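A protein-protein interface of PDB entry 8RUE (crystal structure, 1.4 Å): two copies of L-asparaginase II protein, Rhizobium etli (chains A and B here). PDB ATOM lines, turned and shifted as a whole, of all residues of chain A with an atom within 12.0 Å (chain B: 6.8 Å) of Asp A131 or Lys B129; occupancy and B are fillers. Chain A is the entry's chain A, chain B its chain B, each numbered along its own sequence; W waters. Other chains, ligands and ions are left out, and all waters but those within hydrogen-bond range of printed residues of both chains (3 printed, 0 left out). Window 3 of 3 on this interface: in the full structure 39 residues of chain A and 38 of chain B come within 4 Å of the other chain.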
ATOM      1  N   HIS A 116       6.365   4.218  -0.170  1.00  0.00           N
ATOM      2  CA  HIS A 116       6.805   5.154   0.860  1.00  0.00           C
ATOM      3  C   HIS A 116       7.707   6.215   0.215  1.00  0.00           C
ATOM      4  O   HIS A 116       8.225   6.025  -0.894  1.00  0.00           O
ATOM      5  CB  HIS A 116       7.561   4.414   1.983  1.00  0.00           C
ATOM      6  CG  HIS A 116       8.733   3.640   1.469  1.00  0.00           C
ATOM      7  ND1 HIS A 116       9.931   4.240   1.156  1.00  0.00           N
ATOM      8  CD2 HIS A 116       8.882   2.319   1.188  1.00  0.00           C
ATOM      9  CE1 HIS A 116      10.771   3.323   0.688  1.00  0.00           C
ATOM     10  NE2 HIS A 116      10.158   2.148   0.699  1.00  0.00           N
ATOM     11  N   PRO A 117       7.921   7.334   0.883  1.00  0.00           N
ATOM     12  CA  PRO A 117       8.884   8.309   0.357  1.00  0.00           C
ATOM     13  C   PRO A 117      10.252   7.672   0.201  1.00  0.00           C
ATOM     14  O   PRO A 117      10.690   6.876   1.034  1.00  0.00           O
ATOM     15  CB  PRO A 117       8.896   9.399   1.426  1.00  0.00           C
ATOM     16  CG  PRO A 117       7.566   9.274   2.084  1.00  0.00           C
ATOM     17  CD  PRO A 117       7.237   7.823   2.095  1.00  0.00           C
ATOM     18  N   SER A 118      10.934   8.030  -0.877  1.00  0.00           N
ATOM     19  CA  SER A 118      12.200   7.392  -1.183  1.00  0.00           C
ATOM     20  C   SER A 118      13.213   7.626  -0.074  1.00  0.00           C
ATOM     21  O   SER A 118      13.252   8.686   0.557  1.00  0.00           O
ATOM     22  CB  SER A 118      12.753   7.955  -2.495  1.00  0.00           C
ATOM     23  OG  SER A 118      14.112   7.540  -2.696  1.00  0.00           O
ATOM     24  N   GLU A 121      17.032  11.494  -0.887  1.00  0.00           N
ATOM     25  CA  GLU A 121      16.413  12.806  -0.973  1.00  0.00           C
ATOM     26  C   GLU A 121      16.301  13.281  -2.425  1.00  0.00           C
ATOM     27  O   GLU A 121      15.310  13.922  -2.788  1.00  0.00           O
ATOM     28  CB  GLU A 121      17.155  13.781  -0.050  1.00  0.00           C
ATOM     29  CG  GLU A 121      18.036  14.778  -0.730  1.00  0.00           C
ATOM     30  CD  GLU A 121      17.505  16.191  -0.562  1.00  0.00           C
ATOM     31  OE1 GLU A 121      16.322  16.411  -0.913  1.00  0.00           O
ATOM     32  OE2 GLU A 121      18.251  17.065  -0.064  1.00  0.00           O
ATOM     33  N   MET A 122      17.257  12.910  -3.290  1.00  0.00           N
ATOM     34  CA  MET A 122      17.190  13.369  -4.678  1.00  0.00           C
ATOM     35  C   MET A 122      16.062  12.690  -5.443  1.00  0.00           C
ATOM     36  O   MET A 122      15.376  13.332  -6.250  1.00  0.00           O
ATOM     37  CB  MET A 122      18.530  13.172  -5.391  1.00  0.00           C
ATOM     38  CG  MET A 122      19.622  14.121  -4.919  1.00  0.00           C
ATOM     39  SD  MET A 122      19.200  15.886  -4.989  1.00  0.00           S
ATOM     40  CE  MET A 122      18.866  16.101  -6.738  1.00  0.00           C
ATOM     41  N   VAL A 123      15.853  11.392  -5.210  1.00  0.00           N
ATOM     42  CA  VAL A 123      14.711  10.729  -5.822  1.00  0.00           C
ATOM     43  C   VAL A 123      13.424  11.338  -5.299  1.00  0.00           C
ATOM     44  O   VAL A 123      12.490  11.621  -6.064  1.00  0.00           O
ATOM     45  CB  VAL A 123      14.759   9.210  -5.564  1.00  0.00           C
ATOM     46  CG1 VAL A 123      13.437   8.538  -6.039  1.00  0.00           C
ATOM     47  CG2 VAL A 123      15.967   8.570  -6.258  1.00  0.00           C
ATOM     48  N   ASN A 124      13.349  11.550  -3.982  1.00  0.00           N
ATOM     49  CA  ASN A 124      12.105  12.047  -3.420  1.00  0.00           C
ATOM     50  C   ASN A 124      11.761  13.426  -3.974  1.00  0.00           C
ATOM     51  O   ASN A 124      10.589  13.725  -4.237  1.00  0.00           O
ATOM     52  CB  ASN A 124      12.175  12.067  -1.887  1.00  0.00           C
ATOM     53  CG  ASN A 124      10.839  11.782  -1.262  1.00  0.00           C
ATOM     54  OD1 ASN A 124      10.158  10.819  -1.618  1.00  0.00           O
ATOM     55  ND2 ASN A 124      10.420  12.664  -0.369  1.00  0.00           N
ATOM     56  N   ARG A 125      12.766  14.271  -4.194  1.00  0.00           N
ATOM     57  CA  ARG A 125      12.451  15.596  -4.713  1.00  0.00           C
ATOM     58  C   ARG A 125      11.967  15.525  -6.154  1.00  0.00           C
ATOM     59  O   ARG A 125      11.070  16.282  -6.535  1.00  0.00           O
ATOM     60  CB  ARG A 125      13.601  16.578  -4.494  1.00  0.00           C
ATOM     61  CG  ARG A 125      14.944  16.139  -4.965  1.00  0.00           C
ATOM     62  CD  ARG A 125      16.053  16.880  -4.191  1.00  0.00           C
ATOM     63  NE  ARG A 125      15.835  18.317  -4.074  1.00  0.00           N
ATOM     64  CZ  ARG A 125      15.526  18.952  -2.948  1.00  0.00           C
ATOM     65  NH1 ARG A 125      15.343  18.298  -1.807  1.00  0.00           N
ATOM     66  NH2 ARG A 125      15.407  20.280  -2.964  1.00  0.00           N
ATOM     67  N   SER A 126      12.494  14.584  -6.947  1.00  0.00           N
ATOM     68  CA  SER A 126      11.975  14.409  -8.296  1.00  0.00           C
ATOM     69  C   SER A 126      10.538  13.895  -8.274  1.00  0.00           C
ATOM     70  O   SER A 126       9.712  14.323  -9.090  1.00  0.00           O
ATOM     71  CB  SER A 126      12.893  13.511  -9.125  1.00  0.00           C
ATOM     72  OG  SER A 126      12.856  12.172  -8.682  1.00  0.00           O
ATOM     73  N   TRP A 127      10.211  12.999  -7.338  1.00  0.00           N
ATOM     74  CA  TRP A 127       8.827  12.552  -7.214  1.00  0.00           C
ATOM     75  C   TRP A 127       7.907  13.703  -6.814  1.00  0.00           C
ATOM     76  O   TRP A 127       6.797  13.824  -7.340  1.00  0.00           O
ATOM     77  CB  TRP A 127       8.740  11.452  -6.161  1.00  0.00           C
ATOM     78  CG  TRP A 127       9.343  10.122  -6.561  1.00  0.00           C
ATOM     79  CD1 TRP A 127       9.917   9.784  -7.752  1.00  0.00           C
ATOM     80  CD2 TRP A 127       9.407   8.955  -5.738  1.00  0.00           C
ATOM     81  NE1 TRP A 127      10.337   8.470  -7.720  1.00  0.00           N
ATOM     82  CE2 TRP A 127      10.033   7.944  -6.492  1.00  0.00           C
ATOM     83  CE3 TRP A 127       9.023   8.678  -4.417  1.00  0.00           C
ATOM     84  CZ2 TRP A 127      10.279   6.673  -5.983  1.00  0.00           C
ATOM     85  CZ3 TRP A 127       9.244   7.409  -3.916  1.00  0.00           C
ATOM     86  CH2 TRP A 127       9.875   6.421  -4.699  1.00  0.00           C
ATOM     87  N   ILE A 128       8.336  14.537  -5.857  1.00  0.00           N
ATOM     88  CA  ILE A 128       7.512  15.666  -5.428  1.00  0.00           C
ATOM     89  C   ILE A 128       7.263  16.602  -6.596  1.00  0.00           C
ATOM     90  O   ILE A 128       6.155  17.135  -6.768  1.00  0.00           O
ATOM     91  CB  ILE A 128       8.162  16.398  -4.231  1.00  0.00           C
ATOM     92  CG1 ILE A 128       8.145  15.512  -2.980  1.00  0.00           C
ATOM     93  CG2 ILE A 128       7.442  17.737  -3.951  1.00  0.00           C
ATOM     94  CD1 ILE A 128       9.166  15.897  -1.897  1.00  0.00           C
ATOM     95  N   LYS A 129       8.281  16.798  -7.434  1.00  0.00           N
ATOM     96  CA  LYS A 129       8.153  17.732  -8.547  1.00  0.00           C
ATOM     97  C   LYS A 129       7.173  17.215  -9.587  1.00  0.00           C
ATOM     98  O   LYS A 129       6.507  18.016 -10.254  1.00  0.00           O
ATOM     99  CB  LYS A 129       9.523  17.942  -9.185  1.00  0.00           C
ATOM    100  CG  LYS A 129       9.929  19.370  -9.422  1.00  0.00           C
ATOM    101  CD  LYS A 129      11.443  19.451  -9.573  1.00  0.00           C
ATOM    102  CE  LYS A 129      11.828  20.147 -10.868  1.00  0.00           C
ATOM    103  NZ  LYS A 129      11.050  21.390 -11.079  1.00  0.00           N
ATOM    104  N   GLN A 130       7.079  15.889  -9.740  1.00  0.00           N
ATOM    105  CA  GLN A 130       6.193  15.250 -10.704  1.00  0.00           C
ATOM    106  C   GLN A 130       4.836  14.885 -10.119  1.00  0.00           C
ATOM    107  O   GLN A 130       4.025  14.287 -10.830  1.00  0.00           O
ATOM    108  CB  GLN A 130       6.828  13.968 -11.252  1.00  0.00           C
ATOM    109  CG  GLN A 130       8.101  14.156 -12.043  1.00  0.00           C
ATOM    110  CD  GLN A 130       8.733  12.829 -12.428  1.00  0.00           C
ATOM    111  OE1 GLN A 130       8.636  11.841 -11.695  1.00  0.00           O
ATOM    112  NE2 GLN A 130       9.378  12.798 -13.590  1.00  0.00           N
ATOM    113  N   ASP A 131       4.584  15.184  -8.846  1.00  0.00           N
ATOM    114  CA  ASP A 131       3.361  14.746  -8.163  1.00  0.00           C
ATOM    115  C   ASP A 131       3.217  13.224  -8.175  1.00  0.00           C
ATOM    116  O   ASP A 131       2.119  12.685  -8.296  1.00  0.00           O
ATOM    117  CB  ASP A 131       2.103  15.420  -8.725  1.00  0.00           C
ATOM    118  CG  ASP A 131       2.073  16.901  -8.471  1.00  0.00           C
ATOM    119  OD1 ASP A 131       2.225  17.308  -7.294  1.00  0.00           O
ATOM    120  OD2 ASP A 131       1.891  17.657  -9.454  1.00  0.00           O
ATOM    121  N   PHE A 132       4.324  12.519  -8.041  1.00  0.00           N
ATOM    122  CA  PHE A 132       4.288  11.066  -8.144  1.00  0.00           C
ATOM    123  C   PHE A 132       3.982  10.443  -6.780  1.00  0.00           C
ATOM    124  O   PHE A 132       4.623  10.787  -5.774  1.00  0.00           O
ATOM    125  CB  PHE A 132       5.617  10.542  -8.692  1.00  0.00           C
ATOM    126  CG  PHE A 132       5.712   9.024  -8.713  1.00  0.00           C
ATOM    127  CD1 PHE A 132       4.988   8.268  -9.645  1.00  0.00           C
ATOM    128  CD2 PHE A 132       6.521   8.347  -7.811  1.00  0.00           C
ATOM    129  CE1 PHE A 132       5.069   6.900  -9.670  1.00  0.00           C
ATOM    130  CE2 PHE A 132       6.597   6.961  -7.830  1.00  0.00           C
ATOM    131  CZ  PHE A 132       5.870   6.246  -8.745  1.00  0.00           C
ATOM    132  N   ILE A 133       3.002   9.545  -6.741  1.00  0.00           N
ATOM    133  CA  ILE A 133       2.654   8.808  -5.525  1.00  0.00           C
ATOM    134  C   ILE A 133       3.297   7.427  -5.607  1.00  0.00           C
ATOM    135  O   ILE A 133       2.909   6.631  -6.468  1.00  0.00           O
ATOM    136  CB  ILE A 133       1.136   8.687  -5.337  1.00  0.00           C
ATOM    137  CG1 ILE A 133       0.518  10.068  -5.177  1.00  0.00           C
ATOM    138  CG2 ILE A 133       0.801   7.844  -4.085  1.00  0.00           C
ATOM    139  CD1 ILE A 133      -0.982  10.067  -5.354  1.00  0.00           C
ATOM    140  N   PRO A 134       4.241   7.094  -4.736  1.00  0.00           N
ATOM    141  CA  PRO A 134       4.858   5.766  -4.818  1.00  0.00           C
ATOM    142  C   PRO A 134       3.873   4.653  -4.504  1.00  0.00           C
ATOM    143  O   PRO A 134       2.952   4.796  -3.691  1.00  0.00           O
ATOM    144  CB  PRO A 134       5.997   5.810  -3.791  1.00  0.00           C
ATOM    145  CG  PRO A 134       5.724   6.977  -2.950  1.00  0.00           C
ATOM    146  CD  PRO A 134       4.835   7.929  -3.683  1.00  0.00           C
ATOM    147  N   THR A 135       4.091   3.532  -5.164  1.00  0.00           N
ATOM    148  CA  THR A 135       3.243   2.356  -5.046  1.00  0.00           C
ATOM    149  C   THR A 135       4.107   1.177  -4.619  1.00  0.00           C
ATOM    150  O   THR A 135       5.311   1.322  -4.396  1.00  0.00           O
ATOM    151  CB  THR A 135       2.542   2.045  -6.366  1.00  0.00           C
ATOM    152  OG1 THR A 135       3.522   1.759  -7.374  1.00  0.00           O
ATOM    153  CG2 THR A 135       1.690   3.223  -6.820  1.00  0.00           C
ATOM    154  N   CYS A 138       7.616   0.374  -5.845  1.00  0.00           N
ATOM    155  CA  CYS A 138       8.640   1.323  -5.435  1.00  0.00           C
ATOM    156  C   CYS A 138       9.195   1.060  -4.042  1.00  0.00           C
ATOM    157  O   CYS A 138      10.165   1.728  -3.648  1.00  0.00           O
ATOM    158  CB  CYS A 138       8.062   2.754  -5.420  1.00  0.00           C
ATOM    159  SG  CYS A 138       7.425   3.314  -6.995  1.00  0.00           S
ATOM    160  N   MET B 122       5.199  20.432   4.538  1.00  0.00           N
ATOM    161  CA  MET B 122       4.246  20.888   3.529  1.00  0.00           C
ATOM    162  C   MET B 122       4.746  22.128   2.811  1.00  0.00           C
ATOM    163  O   MET B 122       4.621  22.236   1.586  1.00  0.00           O
ATOM    164  CB  MET B 122       2.880  21.138   4.157  1.00  0.00           C
ATOM    165  CG  MET B 122       2.068  19.852   4.364  1.00  0.00           C
ATOM    166  SD  MET B 122       1.885  18.783   2.893  1.00  0.00           S
ATOM    167  CE  MET B 122       3.176  17.560   3.164  1.00  0.00           C
ATOM    168  N   ASN B 124       7.947  22.919   2.518  1.00  0.00           N
ATOM    169  CA  ASN B 124       9.102  22.505   1.730  1.00  0.00           C
ATOM    170  C   ASN B 124       8.688  21.776   0.457  1.00  0.00           C
ATOM    171  O   ASN B 124       9.328  21.943  -0.584  1.00  0.00           O
ATOM    172  CB  ASN B 124      10.088  21.696   2.577  1.00  0.00           C
ATOM    173  CG  ASN B 124      11.509  21.814   2.061  1.00  0.00           C
ATOM    174  OD1 ASN B 124      12.066  22.913   1.986  1.00  0.00           O
ATOM    175  ND2 ASN B 124      12.078  20.687   1.636  1.00  0.00           N
ATOM    176  N   ARG B 125       7.627  20.953   0.519  1.00  0.00           N
ATOM    177  CA  ARG B 125       7.114  20.316  -0.693  1.00  0.00           C
ATOM    178  C   ARG B 125       6.666  21.354  -1.713  1.00  0.00           C
ATOM    179  O   ARG B 125       6.895  21.195  -2.916  1.00  0.00           O
ATOM    180  CB  ARG B 125       5.943  19.415  -0.309  1.00  0.00           C
ATOM    181  CG  ARG B 125       5.078  18.904  -1.459  1.00  0.00           C
ATOM    182  CD  ARG B 125       4.042  17.946  -0.886  1.00  0.00           C
ATOM    183  NE  ARG B 125       4.605  17.333   0.312  1.00  0.00           N
ATOM    184  CZ  ARG B 125       5.223  16.161   0.342  1.00  0.00           C
ATOM    185  NH1 ARG B 125       5.205  15.341  -0.701  1.00  0.00           N
ATOM    186  NH2 ARG B 125       5.879  15.803   1.445  1.00  0.00           N
ATOM    187  N   SER B 126       5.973  22.397  -1.258  1.00  0.00           N
ATOM    188  CA  SER B 126       5.561  23.451  -2.171  1.00  0.00           C
ATOM    189  C   SER B 126       6.772  24.137  -2.800  1.00  0.00           C
ATOM    190  O   SER B 126       6.787  24.390  -4.010  1.00  0.00           O
ATOM    191  CB  SER B 126       4.695  24.457  -1.421  1.00  0.00           C
ATOM    192  OG  SER B 126       4.157  25.400  -2.314  1.00  0.00           O
ATOM    193  N   TRP B 127       7.815  24.407  -2.003  1.00  0.00           N
ATOM    194  CA  TRP B 127       9.027  25.012  -2.558  1.00  0.00           C
ATOM    195  C   TRP B 127       9.674  24.112  -3.600  1.00  0.00           C
ATOM    196  O   TRP B 127      10.153  24.595  -4.632  1.00  0.00           O
ATOM    197  CB  TRP B 127      10.029  25.278  -1.442  1.00  0.00           C
ATOM    198  CG  TRP B 127       9.630  26.387  -0.505  1.00  0.00           C
ATOM    199  CD1 TRP B 127       8.495  27.129  -0.536  1.00  0.00           C
ATOM    200  CD2 TRP B 127      10.382  26.837   0.615  1.00  0.00           C
ATOM    201  NE1 TRP B 127       8.488  28.036   0.500  1.00  0.00           N
ATOM    202  CE2 TRP B 127       9.648  27.879   1.219  1.00  0.00           C
ATOM    203  CE3 TRP B 127      11.607  26.455   1.176  1.00  0.00           C
ATOM    204  CZ2 TRP B 127      10.113  28.566   2.332  1.00  0.00           C
ATOM    205  CZ3 TRP B 127      12.065  27.135   2.294  1.00  0.00           C
ATOM    206  CH2 TRP B 127      11.311  28.165   2.868  1.00  0.00           C
ATOM    207  N   ILE B 128       9.752  22.808  -3.327  1.00  0.00           N
ATOM    208  CA  ILE B 128      10.335  21.884  -4.296  1.00  0.00           C
ATOM    209  C   ILE B 128       9.556  21.905  -5.611  1.00  0.00           C
ATOM    210  O   ILE B 128      10.149  21.924  -6.697  1.00  0.00           O
ATOM    211  CB  ILE B 128      10.425  20.472  -3.688  1.00  0.00           C
ATOM    212  CG1 ILE B 128      11.505  20.435  -2.603  1.00  0.00           C
ATOM    213  CG2 ILE B 128      10.746  19.469  -4.784  1.00  0.00           C
ATOM    214  CD1 ILE B 128      11.456  19.232  -1.689  1.00  0.00           C
ATOM    215  N   LYS B 129       8.220  21.902  -5.536  1.00  0.00           N
ATOM    216  CA  LYS B 129       7.413  21.902  -6.757  1.00  0.00           C
ATOM    217  C   LYS B 129       7.631  23.165  -7.577  1.00  0.00           C
ATOM    218  O   LYS B 129       7.495  23.136  -8.809  1.00  0.00           O
ATOM    219  CB  LYS B 129       5.923  21.794  -6.438  1.00  0.00           C
ATOM    220  CG  LYS B 129       5.438  20.444  -6.010  1.00  0.00           C
ATOM    221  CD  LYS B 129       3.920  20.392  -5.955  1.00  0.00           C
ATOM    222  CE  LYS B 129       3.413  20.406  -4.517  1.00  0.00           C
ATOM    223  NZ  LYS B 129       2.967  19.056  -4.043  1.00  0.00           N
ATOM    224  N   GLN B 130       7.957  24.273  -6.917  1.00  0.00           N
ATOM    225  CA  GLN B 130       8.138  25.578  -7.547  1.00  0.00           C
ATOM    226  C   GLN B 130       9.589  25.886  -7.897  1.00  0.00           C
ATOM    227  O   GLN B 130       9.850  26.956  -8.451  1.00  0.00           O
ATOM    228  CB  GLN B 130       7.647  26.691  -6.615  1.00  0.00           C
ATOM    229  CG  GLN B 130       6.217  26.575  -6.189  1.00  0.00           C
ATOM    230  CD  GLN B 130       5.832  27.700  -5.240  1.00  0.00           C
ATOM    231  OE1 GLN B 130       6.432  28.779  -5.259  1.00  0.00           O
ATOM    232  NE2 GLN B 130       4.843  27.443  -4.392  1.00  0.00           N
ATOM    233  N   ASP B 131      10.534  25.001  -7.573  1.00  0.00           N
ATOM    234  CA  ASP B 131      11.968  25.301  -7.698  1.00  0.00           C
ATOM    235  C   ASP B 131      12.354  26.566  -6.940  1.00  0.00           C
ATOM    236  O   ASP B 131      13.202  27.347  -7.380  1.00  0.00           O
ATOM    237  CB  ASP B 131      12.415  25.386  -9.154  1.00  0.00           C
ATOM    238  CG  ASP B 131      12.180  24.106  -9.899  1.00  0.00           C
ATOM    239  OD1 ASP B 131      12.655  23.054  -9.428  1.00  0.00           O
ATOM    240  OD2 ASP B 131      11.503  24.151 -10.940  1.00  0.00           O
ATOM    241  N   PHE B 132      11.716  26.777  -5.799  1.00  0.00           N
ATOM    242  CA  PHE B 132      11.985  27.963  -4.994  1.00  0.00           C
ATOM    243  C   PHE B 132      13.301  27.819  -4.234  1.00  0.00           C
ATOM    244  O   PHE B 132      13.562  26.791  -3.593  1.00  0.00           O
ATOM    245  CB  PHE B 132      10.840  28.205  -4.007  1.00  0.00           C
ATOM    246  CG  PHE B 132      11.063  29.399  -3.110  1.00  0.00           C
ATOM    247  CD1 PHE B 132      10.995  30.702  -3.606  1.00  0.00           C
ATOM    248  CD2 PHE B 132      11.346  29.217  -1.758  1.00  0.00           C
ATOM    249  CE1 PHE B 132      11.207  31.792  -2.757  1.00  0.00           C
ATOM    250  CE2 PHE B 132      11.549  30.308  -0.899  1.00  0.00           C
ATOM    251  CZ  PHE B 132      11.497  31.591  -1.403  1.00  0.00           C
HETATM  252  O   HOH W   1       3.996  16.763  -5.136  1.00  0.00           O
HETATM  253  O   HOH W   2      14.730  20.557   0.447  1.00  0.00           O
HETATM  254  O   HOH W   3       7.660  13.032   0.948  1.00  0.00           O
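Of the printed residues of chain B, Arg A125 touches Ile B128 (3.7 Å).
Printed residues of chain B within 4 Å of Ile A128: Arg B125, Ile B128 and Lys B129.
Of the printed residues of chain B, Lys A129 touches Ile B128 (3.7 Å) and Asp B131 (2.8 Å).
Of the printed residues of chain B, Asp A131 touches Lys B129.
Printed residues of chain A within 4 Å of Arg B125: Ile A128.
Of chain A, only Arg A125 (3.7 Å), Ile A128 (3.8 Å) and Lys A129 (3.7 Å) come within 4 Å of Ile B128.
Lys B129 touches just these residues of chain A: Ile A128 and Asp A131.
The nearest residue of chain B that does not touch Asp A131 is Arg B125 (6.7 Å).
The nearest printed residue of chain B that does not touch Ile A128 is Ser B126 (5.6 Å).
Arg A125 touches Ile B128, and with the chains exchanged Ile A128 touches Arg B125.
Ile A128 touches its own counterpart, Ile B128.
Ile A128 touches Lys B129, and with the chains exchanged Lys A129 touches Ile B128.
Lys A129 touches Asp B131, and with the chains exchanged Asp A131 touches Lys B129.
Positions printed for both chains: 122, 124, 125, 126, 127, 128, 129, 130, 131 and 132.
Of the 7 pairs that touch across the chains among the printed residues, 7 have their exchanged pair printed and touching as well.
Among the printed residues, pairs that only touch across the chains: Arg A125 with Ile B128, Ile A128 with Arg B125, Ile A128 with Ile B128, Ile A128 with Lys B129 and Lys A129 with Ile B128.
The side-chain carboxylate (OD1) of Asp A131 lies within salt-bridge range of the side-chain amino group (NZ) of Lys B129 (3.8 Å).
OD2 of Asp B131 lies within salt-bridge range of NZ of Lys A129 (2.8 Å).
Of the 19 printed residues of chain A, 4 touch a printed residue of chain B.
Hydrophobic or aromatic side chains of chain A that line the printed part of chain B: Ile A128.
Hydrophobic or aromatic side chains of chain B within 4 Å of the printed part of chain A: Ile B128.
Among the printed residues, 7 pairs touch across the chains.
Among the printed residues, Asp or Glu carboxylates within 4 Å of a Lys or Arg side-chain nitrogen of the other chain: Lys A129 with Asp B131 (2.8 Å) and Asp A131 with Lys B129 (3.8 Å).
Water W1 lies within hydrogen-bond range of the backbone carbonyl oxygen of Ile A128, the side-chain amino group of Lys B129 and the side-chain carboxylate of Asp A131.
Water W2 lies within hydrogen-bond range of ND2 of Asn B124 (2.9 Å) and NH1 of Arg A125 (3.2 Å).
Water W3 lies within hydrogen-bond range of the side-chain amide nitrogen (ND2) of Asn A124 (3.1 Å) and the guanidinium group (NH2) of Arg B125 (3.3 Å).
OE2 of Glu A121 is in salt-bridge range of NH1 of Arg A125 (3.6 Å).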
